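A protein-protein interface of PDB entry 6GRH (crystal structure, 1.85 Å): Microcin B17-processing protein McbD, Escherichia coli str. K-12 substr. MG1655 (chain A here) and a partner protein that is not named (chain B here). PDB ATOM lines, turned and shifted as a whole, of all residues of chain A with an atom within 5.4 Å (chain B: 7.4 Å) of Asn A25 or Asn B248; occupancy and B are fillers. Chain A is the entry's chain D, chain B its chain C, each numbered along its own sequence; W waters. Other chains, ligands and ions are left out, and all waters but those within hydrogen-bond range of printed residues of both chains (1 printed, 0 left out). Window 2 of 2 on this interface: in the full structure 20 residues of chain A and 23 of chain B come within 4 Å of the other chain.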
ATOM      1  N   LEU A  22       0.121 -30.475  18.599  1.00  0.00           N
ATOM      2  CA  LEU A  22       0.036 -30.644  17.157  1.00  0.00           C
ATOM      3  C   LEU A  22      -0.577 -29.430  16.450  1.00  0.00           C
ATOM      4  O   LEU A  22      -0.134 -29.077  15.363  1.00  0.00           O
ATOM      5  CB  LEU A  22      -0.767 -31.887  16.800  1.00  0.00           C
ATOM      6  CG  LEU A  22      -0.241 -33.257  17.219  1.00  0.00           C
ATOM      7  CD1 LEU A  22      -1.100 -34.355  16.622  1.00  0.00           C
ATOM      8  CD2 LEU A  22       1.200 -33.449  16.778  1.00  0.00           C
ATOM      9  N   ASN A  23      -1.575 -28.819  17.086  1.00  0.00           N
ATOM     10  CA  ASN A  23      -2.429 -27.770  16.509  1.00  0.00           C
ATOM     11  C   ASN A  23      -1.878 -26.365  16.819  1.00  0.00           C
ATOM     12  O   ASN A  23      -1.843 -25.932  17.988  1.00  0.00           O
ATOM     13  CB  ASN A  23      -3.833 -27.924  17.113  1.00  0.00           C
ATOM     14  CG  ASN A  23      -4.848 -26.996  16.502  1.00  0.00           C
ATOM     15  OD1 ASN A  23      -4.509 -26.065  15.770  1.00  0.00           O
ATOM     16  ND2 ASN A  23      -6.116 -27.252  16.796  1.00  0.00           N
ATOM     17  N   ARG A  24      -1.463 -25.646  15.781  1.00  0.00           N
ATOM     18  CA  ARG A  24      -0.886 -24.321  15.960  1.00  0.00           C
ATOM     19  C   ARG A  24      -1.898 -23.317  16.521  1.00  0.00           C
ATOM     20  O   ARG A  24      -1.504 -22.337  17.154  1.00  0.00           O
ATOM     21  CB  ARG A  24      -0.270 -23.783  14.658  1.00  0.00           C
ATOM     22  CG  ARG A  24      -1.262 -23.318  13.621  1.00  0.00           C
ATOM     23  CD  ARG A  24      -0.585 -22.868  12.344  1.00  0.00           C
ATOM     24  NE  ARG A  24      -1.534 -22.147  11.516  1.00  0.00           N
ATOM     25  CZ  ARG A  24      -1.813 -20.846  11.630  1.00  0.00           C
ATOM     26  NH1 ARG A  24      -1.178 -20.073  12.511  1.00  0.00           N
ATOM     27  NH2 ARG A  24      -2.711 -20.301  10.827  1.00  0.00           N
ATOM     28  N   ASN A  25      -3.176 -23.596  16.298  1.00  0.00           N
ATOM     29  CA  ASN A  25      -4.257 -22.798  16.844  1.00  0.00           C
ATOM     30  C   ASN A  25      -4.750 -23.128  18.240  1.00  0.00           C
ATOM     31  O   ASN A  25      -5.667 -22.483  18.706  1.00  0.00           O
ATOM     32  CB  ASN A  25      -5.422 -22.775  15.840  1.00  0.00           C
ATOM     33  CG  ASN A  25      -5.052 -22.042  14.580  1.00  0.00           C
ATOM     34  OD1 ASN A  25      -4.485 -20.956  14.663  1.00  0.00           O
ATOM     35  ND2 ASN A  25      -5.313 -22.639  13.419  1.00  0.00           N
ATOM     36  N   MET A  26      -4.176 -24.110  18.929  1.00  0.00           N
ATOM     37  CA  MET A  26      -4.531 -24.304  20.325  1.00  0.00           C
ATOM     38  C   MET A  26      -3.585 -23.461  21.172  1.00  0.00           C
ATOM     39  O   MET A  26      -2.478 -23.138  20.726  1.00  0.00           O
ATOM     40  CB  MET A  26      -4.518 -25.772  20.728  1.00  0.00           C
ATOM     41  CG  MET A  26      -5.779 -26.542  20.278  1.00  0.00           C
ATOM     42  SD  MET A  26      -7.295 -26.050  21.143  1.00  0.00           S
ATOM     43  CE  MET A  26      -8.519 -27.263  20.610  1.00  0.00           C
ATOM     44  N   PRO A  27      -4.021 -23.071  22.382  1.00  0.00           N
ATOM     45  CA  PRO A  27      -3.129 -22.321  23.273  1.00  0.00           C
ATOM     46  C   PRO A  27      -1.943 -23.175  23.704  1.00  0.00           C
ATOM     47  O   PRO A  27      -2.019 -24.381  23.692  1.00  0.00           O
ATOM     48  CB  PRO A  27      -4.004 -21.950  24.471  1.00  0.00           C
ATOM     49  CG  PRO A  27      -5.294 -22.650  24.311  1.00  0.00           C
ATOM     50  CD  PRO A  27      -5.376 -23.243  22.936  1.00  0.00           C
ATOM     51  N   ASN A 196      -8.107 -16.536  16.874  1.00  0.00           N
ATOM     52  CA  ASN A 196      -8.092 -17.925  16.407  1.00  0.00           C
ATOM     53  C   ASN A 196      -8.101 -18.964  17.546  1.00  0.00           C
ATOM     54  O   ASN A 196      -8.889 -19.903  17.491  1.00  0.00           O
ATOM     55  CB  ASN A 196      -6.906 -18.199  15.448  1.00  0.00           C
ATOM     56  CG  ASN A 196      -7.213 -17.801  14.008  1.00  0.00           C
ATOM     57  OD1 ASN A 196      -8.195 -17.116  13.729  1.00  0.00           O
ATOM     58  ND2 ASN A 196      -6.388 -18.259  13.085  1.00  0.00           N
ATOM     59  N   HIS A 197      -7.289 -18.775  18.571  1.00  0.00           N
ATOM     60  CA  HIS A 197      -7.216 -19.790  19.632  1.00  0.00           C
ATOM     61  C   HIS A 197      -8.454 -19.818  20.529  1.00  0.00           C
ATOM     62  O   HIS A 197      -8.795 -20.872  21.057  1.00  0.00           O
ATOM     63  CB  HIS A 197      -5.899 -19.769  20.418  1.00  0.00           C
ATOM     64  CG  HIS A 197      -5.714 -18.592  21.330  1.00  0.00           C
ATOM     65  ND1 HIS A 197      -5.262 -17.364  20.887  1.00  0.00           N
ATOM     66  CD2 HIS A 197      -5.866 -18.474  22.670  1.00  0.00           C
ATOM     67  CE1 HIS A 197      -5.158 -16.540  21.918  1.00  0.00           C
ATOM     68  NE2 HIS A 197      -5.524 -17.186  23.010  1.00  0.00           N
ATOM     69  N   GLU A 200     -11.227 -21.560  18.336  1.00  0.00           N
ATOM     70  CA  GLU A 200     -10.890 -22.988  18.302  1.00  0.00           C
ATOM     71  C   GLU A 200     -11.414 -23.719  19.565  1.00  0.00           C
ATOM     72  O   GLU A 200     -12.051 -24.769  19.458  1.00  0.00           O
ATOM     73  CB  GLU A 200      -9.375 -23.147  18.186  1.00  0.00           C
ATOM     74  CG  GLU A 200      -8.897 -24.537  17.817  1.00  0.00           C
ATOM     75  CD  GLU A 200      -8.731 -24.759  16.325  1.00  0.00           C
ATOM     76  OE1 GLU A 200      -9.180 -23.931  15.486  1.00  0.00           O
ATOM     77  OE2 GLU A 200      -8.151 -25.810  15.995  1.00  0.00           O
ATOM     78  N   PHE B 132      -1.849 -37.931   8.316  1.00  0.00           N
ATOM     79  CA  PHE B 132      -2.886 -36.976   8.013  1.00  0.00           C
ATOM     80  C   PHE B 132      -3.415 -37.241   6.601  1.00  0.00           C
ATOM     81  O   PHE B 132      -2.667 -37.646   5.713  1.00  0.00           O
ATOM     82  CB  PHE B 132      -2.338 -35.565   8.137  1.00  0.00           C
ATOM     83  CG  PHE B 132      -2.082 -35.124   9.561  1.00  0.00           C
ATOM     84  CD1 PHE B 132      -0.896 -35.437  10.193  1.00  0.00           C
ATOM     85  CD2 PHE B 132      -3.036 -34.387  10.264  1.00  0.00           C
ATOM     86  CE1 PHE B 132      -0.643 -35.009  11.502  1.00  0.00           C
ATOM     87  CE2 PHE B 132      -2.801 -33.961  11.571  1.00  0.00           C
ATOM     88  CZ  PHE B 132      -1.613 -34.295  12.202  1.00  0.00           C
ATOM     89  N   VAL B 149      -8.754 -31.653   5.712  1.00  0.00           N
ATOM     90  CA  VAL B 149      -7.633 -32.324   6.362  1.00  0.00           C
ATOM     91  C   VAL B 149      -8.188 -33.068   7.560  1.00  0.00           C
ATOM     92  O   VAL B 149      -8.985 -32.514   8.301  1.00  0.00           O
ATOM     93  CB  VAL B 149      -6.559 -31.336   6.834  1.00  0.00           C
ATOM     94  CG1 VAL B 149      -5.372 -32.088   7.378  1.00  0.00           C
ATOM     95  CG2 VAL B 149      -6.111 -30.436   5.693  1.00  0.00           C
ATOM     96  N   VAL B 162      -9.244 -31.863  11.166  1.00  0.00           N
ATOM     97  CA  VAL B 162      -8.080 -31.012  11.384  1.00  0.00           C
ATOM     98  C   VAL B 162      -8.216 -29.613  10.792  1.00  0.00           C
ATOM     99  O   VAL B 162      -7.907 -28.647  11.486  1.00  0.00           O
ATOM    100  CB  VAL B 162      -6.805 -31.716  10.886  1.00  0.00           C
ATOM    101  CG1 VAL B 162      -5.591 -30.782  10.873  1.00  0.00           C
ATOM    102  CG2 VAL B 162      -6.525 -32.941  11.754  1.00  0.00           C
ATOM    103  N   ALA B 163      -8.635 -29.480   9.533  1.00  0.00           N
ATOM    104  CA  ALA B 163      -8.660 -28.166   8.865  1.00  0.00           C
ATOM    105  C   ALA B 163      -9.731 -28.056   7.797  1.00  0.00           C
ATOM    106  O   ALA B 163     -10.076 -29.033   7.136  1.00  0.00           O
ATOM    107  CB  ALA B 163      -7.304 -27.843   8.261  1.00  0.00           C
ATOM    108  N   THR B 164     -10.242 -26.840   7.653  1.00  0.00           N
ATOM    109  CA  THR B 164     -11.218 -26.488   6.653  1.00  0.00           C
ATOM    110  C   THR B 164     -10.605 -25.600   5.562  1.00  0.00           C
ATOM    111  O   THR B 164     -11.309 -24.777   4.985  1.00  0.00           O
ATOM    112  CB  THR B 164     -12.367 -25.710   7.314  1.00  0.00           C
ATOM    113  OG1 THR B 164     -11.834 -24.535   7.926  1.00  0.00           O
ATOM    114  CG2 THR B 164     -13.057 -26.541   8.389  1.00  0.00           C
ATOM    115  N   CYS B 165      -9.315 -25.742   5.272  1.00  0.00           N
ATOM    116  CA  CYS B 165      -8.731 -25.057   4.112  1.00  0.00           C
ATOM    117  C   CYS B 165      -9.357 -25.639   2.851  1.00  0.00           C
ATOM    118  O   CYS B 165      -9.785 -26.803   2.856  1.00  0.00           O
ATOM    119  CB  CYS B 165      -7.227 -25.233   4.056  1.00  0.00           C
ATOM    120  SG  CYS B 165      -6.681 -26.932   4.330  1.00  0.00           S
ATOM    121  N   TYR B 242       5.147 -24.703   4.433  1.00  0.00           N
ATOM    122  CA  TYR B 242       3.896 -24.285   3.818  1.00  0.00           C
ATOM    123  C   TYR B 242       2.822 -25.387   3.957  1.00  0.00           C
ATOM    124  O   TYR B 242       1.676 -25.095   4.289  1.00  0.00           O
ATOM    125  CB  TYR B 242       4.176 -23.975   2.356  1.00  0.00           C
ATOM    126  CG  TYR B 242       3.053 -23.458   1.501  1.00  0.00           C
ATOM    127  CD1 TYR B 242       1.996 -22.726   2.022  1.00  0.00           C
ATOM    128  CD2 TYR B 242       3.105 -23.639   0.117  1.00  0.00           C
ATOM    129  CE1 TYR B 242       0.997 -22.217   1.189  1.00  0.00           C
ATOM    130  CE2 TYR B 242       2.108 -23.175  -0.713  1.00  0.00           C
ATOM    131  CZ  TYR B 242       1.064 -22.465  -0.177  1.00  0.00           C
ATOM    132  OH  TYR B 242       0.109 -21.980  -1.045  1.00  0.00           O
ATOM    133  N   VAL B 243       3.215 -26.631   3.736  1.00  0.00           N
ATOM    134  CA  VAL B 243       2.344 -27.784   4.031  1.00  0.00           C
ATOM    135  C   VAL B 243       1.921 -27.772   5.516  1.00  0.00           C
ATOM    136  O   VAL B 243       0.714 -27.826   5.828  1.00  0.00           O
ATOM    137  CB  VAL B 243       3.037 -29.105   3.664  1.00  0.00           C
ATOM    138  CG1 VAL B 243       2.255 -30.317   4.175  1.00  0.00           C
ATOM    139  CG2 VAL B 243       3.206 -29.170   2.144  1.00  0.00           C
ATOM    140  N   ALA B 244       2.892 -27.617   6.417  1.00  0.00           N
ATOM    141  CA  ALA B 244       2.586 -27.560   7.850  1.00  0.00           C
ATOM    142  C   ALA B 244       1.569 -26.453   8.195  1.00  0.00           C
ATOM    143  O   ALA B 244       0.588 -26.707   8.884  1.00  0.00           O
ATOM    144  CB  ALA B 244       3.848 -27.421   8.685  1.00  0.00           C
ATOM    145  N   LYS B 245       1.806 -25.243   7.686  1.00  0.00           N
ATOM    146  CA  LYS B 245       0.964 -24.079   7.955  1.00  0.00           C
ATOM    147  C   LYS B 245      -0.468 -24.318   7.441  1.00  0.00           C
ATOM    148  O   LYS B 245      -1.461 -24.043   8.152  1.00  0.00           O
ATOM    149  CB  LYS B 245       1.566 -22.855   7.271  1.00  0.00           C
ATOM    150  CG  LYS B 245       0.778 -21.543   7.345  1.00  0.00           C
ATOM    151  CD  LYS B 245       1.003 -20.841   8.679  1.00  0.00           C
ATOM    152  CE  LYS B 245       0.190 -19.541   8.755  1.00  0.00           C
ATOM    153  NZ  LYS B 245       0.999 -18.428   9.345  1.00  0.00           N
ATOM    154  N   THR B 246      -0.553 -24.876   6.229  1.00  0.00           N
ATOM    155  CA  THR B 246      -1.835 -25.114   5.544  1.00  0.00           C
ATOM    156  C   THR B 246      -2.687 -26.140   6.295  1.00  0.00           C
ATOM    157  O   THR B 246      -3.894 -25.994   6.411  1.00  0.00           O
ATOM    158  CB  THR B 246      -1.594 -25.526   4.067  1.00  0.00           C
ATOM    159  OG1 THR B 246      -0.880 -24.474   3.420  1.00  0.00           O
ATOM    160  CG2 THR B 246      -2.896 -25.720   3.307  1.00  0.00           C
ATOM    161  N   MET B 247      -2.023 -27.135   6.852  1.00  0.00           N
ATOM    162  CA  MET B 247      -2.639 -28.139   7.730  1.00  0.00           C
ATOM    163  C   MET B 247      -2.839 -27.693   9.200  1.00  0.00           C
ATOM    164  O   MET B 247      -3.347 -28.472  10.017  1.00  0.00           O
ATOM    165  CB  MET B 247      -1.804 -29.417   7.682  1.00  0.00           C
ATOM    166  CG  MET B 247      -1.815 -30.080   6.306  1.00  0.00           C
ATOM    167  SD  MET B 247      -0.653 -31.465   6.206  1.00  0.00           S
ATOM    168  CE  MET B 247      -1.462 -32.639   7.247  1.00  0.00           C
ATOM    169  N   ASN B 248      -2.450 -26.461   9.520  1.00  0.00           N
ATOM    170  CA  ASN B 248      -2.467 -25.913  10.866  1.00  0.00           C
ATOM    171  C   ASN B 248      -1.624 -26.727  11.868  1.00  0.00           C
ATOM    172  O   ASN B 248      -1.944 -26.795  13.053  1.00  0.00           O
ATOM    173  CB  ASN B 248      -3.911 -25.714  11.356  1.00  0.00           C
ATOM    174  CG  ASN B 248      -4.600 -24.572  10.642  1.00  0.00           C
ATOM    175  OD1 ASN B 248      -4.012 -23.510  10.456  1.00  0.00           O
ATOM    176  ND2 ASN B 248      -5.826 -24.784  10.238  1.00  0.00           N
ATOM    177  N   LEU B 249      -0.529 -27.305  11.394  1.00  0.00           N
ATOM    178  CA  LEU B 249       0.396 -27.997  12.288  1.00  0.00           C
ATOM    179  C   LEU B 249       1.327 -26.977  12.950  1.00  0.00           C
ATOM    180  O   LEU B 249       1.738 -25.999  12.309  1.00  0.00           O
ATOM    181  CB  LEU B 249       1.235 -29.010  11.530  1.00  0.00           C
ATOM    182  CG  LEU B 249       0.544 -30.160  10.794  1.00  0.00           C
ATOM    183  CD1 LEU B 249       1.609 -31.046  10.155  1.00  0.00           C
ATOM    184  CD2 LEU B 249      -0.310 -30.965  11.715  1.00  0.00           C
ATOM    185  N   ASP B 250       1.715 -27.242  14.193  1.00  0.00           N
ATOM    186  CA  ASP B 250       2.701 -26.433  14.908  1.00  0.00           C
ATOM    187  C   ASP B 250       4.100 -27.019  14.682  1.00  0.00           C
ATOM    188  O   ASP B 250       4.460 -28.072  15.253  1.00  0.00           O
ATOM    189  CB  ASP B 250       2.373 -26.389  16.387  1.00  0.00           C
ATOM    190  CG  ASP B 250       3.198 -25.320  17.166  1.00  0.00           C
ATOM    191  OD1 ASP B 250       4.363 -24.981  16.819  1.00  0.00           O
ATOM    192  OD2 ASP B 250       2.653 -24.817  18.181  1.00  0.00           O
ATOM    193  N   GLN B 251       4.879 -26.312  13.853  1.00  0.00           N
ATOM    194  CA  GLN B 251       6.218 -26.753  13.445  1.00  0.00           C
ATOM    195  C   GLN B 251       7.233 -26.870  14.552  1.00  0.00           C
ATOM    196  O   GLN B 251       8.245 -27.515  14.351  1.00  0.00           O
ATOM    197  CB  GLN B 251       6.773 -25.839  12.356  1.00  0.00           C
ATOM    198  CG  GLN B 251       6.116 -26.075  11.005  1.00  0.00           C
ATOM    199  CD  GLN B 251       6.540 -25.016  10.020  1.00  0.00           C
ATOM    200  OE1 GLN B 251       7.627 -25.114   9.486  1.00  0.00           O
ATOM    201  NE2 GLN B 251       5.734 -23.963   9.853  1.00  0.00           N
ATOM    202  N   VAL B 254       5.790 -30.691  15.410  1.00  0.00           N
ATOM    203  CA  VAL B 254       5.499 -31.692  14.383  1.00  0.00           C
ATOM    204  C   VAL B 254       5.879 -31.178  12.979  1.00  0.00           C
ATOM    205  O   VAL B 254       5.737 -29.981  12.677  1.00  0.00           O
ATOM    206  CB  VAL B 254       4.032 -32.199  14.491  1.00  0.00           C
ATOM    207  CG1 VAL B 254       3.015 -31.073  14.401  1.00  0.00           C
ATOM    208  CG2 VAL B 254       3.704 -33.262  13.459  1.00  0.00           C
HETATM  209  O   HOH W   1      -3.223 -21.967   7.946  1.00  0.00           O
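The backbone carbonyl oxygen (O) of Leu A22 sits at hydrogen-bond distance from the backbone NH (N) of Asp B250, at 2.9 Å. OD1 of Asn B248 sits at hydrogen-bond distance from ND2 of Asn A25. The backbone carbonyl oxygen of Asn B248 lies within hydrogen-bond range of the backbone NH of Arg A24 (3.0 Å).
OD1 of Asn A23 lies within hydrogen-bond range of N of Asn A25. The backbone NH (N) of Leu B249 is in hydrogen-bond range of the backbone carbonyl oxygen (O) of Ala B244, 2.8 Å away. The side-chain amide nitrogen (ND2) of Asn A23 lies within hydrogen-bond range of the side-chain carboxylate (OE2) of Glu A200 (2.6 Å). The side-chain amide oxygen (OD1) of Asn B248 sits close to the backbone carbonyl oxygen (O) of Lys B245 (3.5 Å).
Water W1 lies within hydrogen-bond range of the backbone carbonyl oxygen (O) of Lys B245 (2.7 Å), the side-chain amide oxygen (OD1) of Asn B248 (3.1 Å) and the guanidinium group (NH2) of Arg A24 (3.4 Å).
Of the 17 printed residues of chain B, 5 touch a printed residue of chain A. Along chain B the printed residues that touch a printed residue of chain A span positions 245 to 254. Hydrophobic or aromatic side chains of chain A within 4 Å of the printed part of chain B: Leu A22. Among the printed residues, no Asp or Glu carboxylate lies within 4 Å of a Lys or Arg side-chain nitrogen of the other chain.
Asn A25 touches just one residue of chain B: Asn B248 (3.4 Å). Printed residues of chain A within 4 Å of Lys B245: Arg A24. Thr B246 touches none of the printed residues of chain A. Met B247 touches none of the printed residues of chain A. Asn B248 touches just these residues of chain A: Leu A22 (3.7 Å), Asn A23 (3.6 Å), Arg A24 (3.0 Å) and Asn A25 (3.4 Å). Of the printed residues of chain A, Leu B249 touches Leu A22 (3.3 Å) and Arg A24 (3.8 Å). The nearest printed residue of chain A that does not touch Asn B248 is Glu A200 (6.3 Å). The nearest printed residue of chain B that does not touch Arg A24 is Ala B244 (5.3 Å).
Among the printed residues, merely in contact across the chains: Leu A22 with Leu B249 (3.3 Å), Asn A23 with Asn B248 (3.6 Å), Arg A24 with Lys B245 (3.6 Å), Leu A22 with Asn B248 (3.7 Å), Arg A24 with Leu B249 (3.8 Å), Leu A22 with Val B254 (3.8 Å) and Arg A24 with Asp B250 (3.9 Å).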
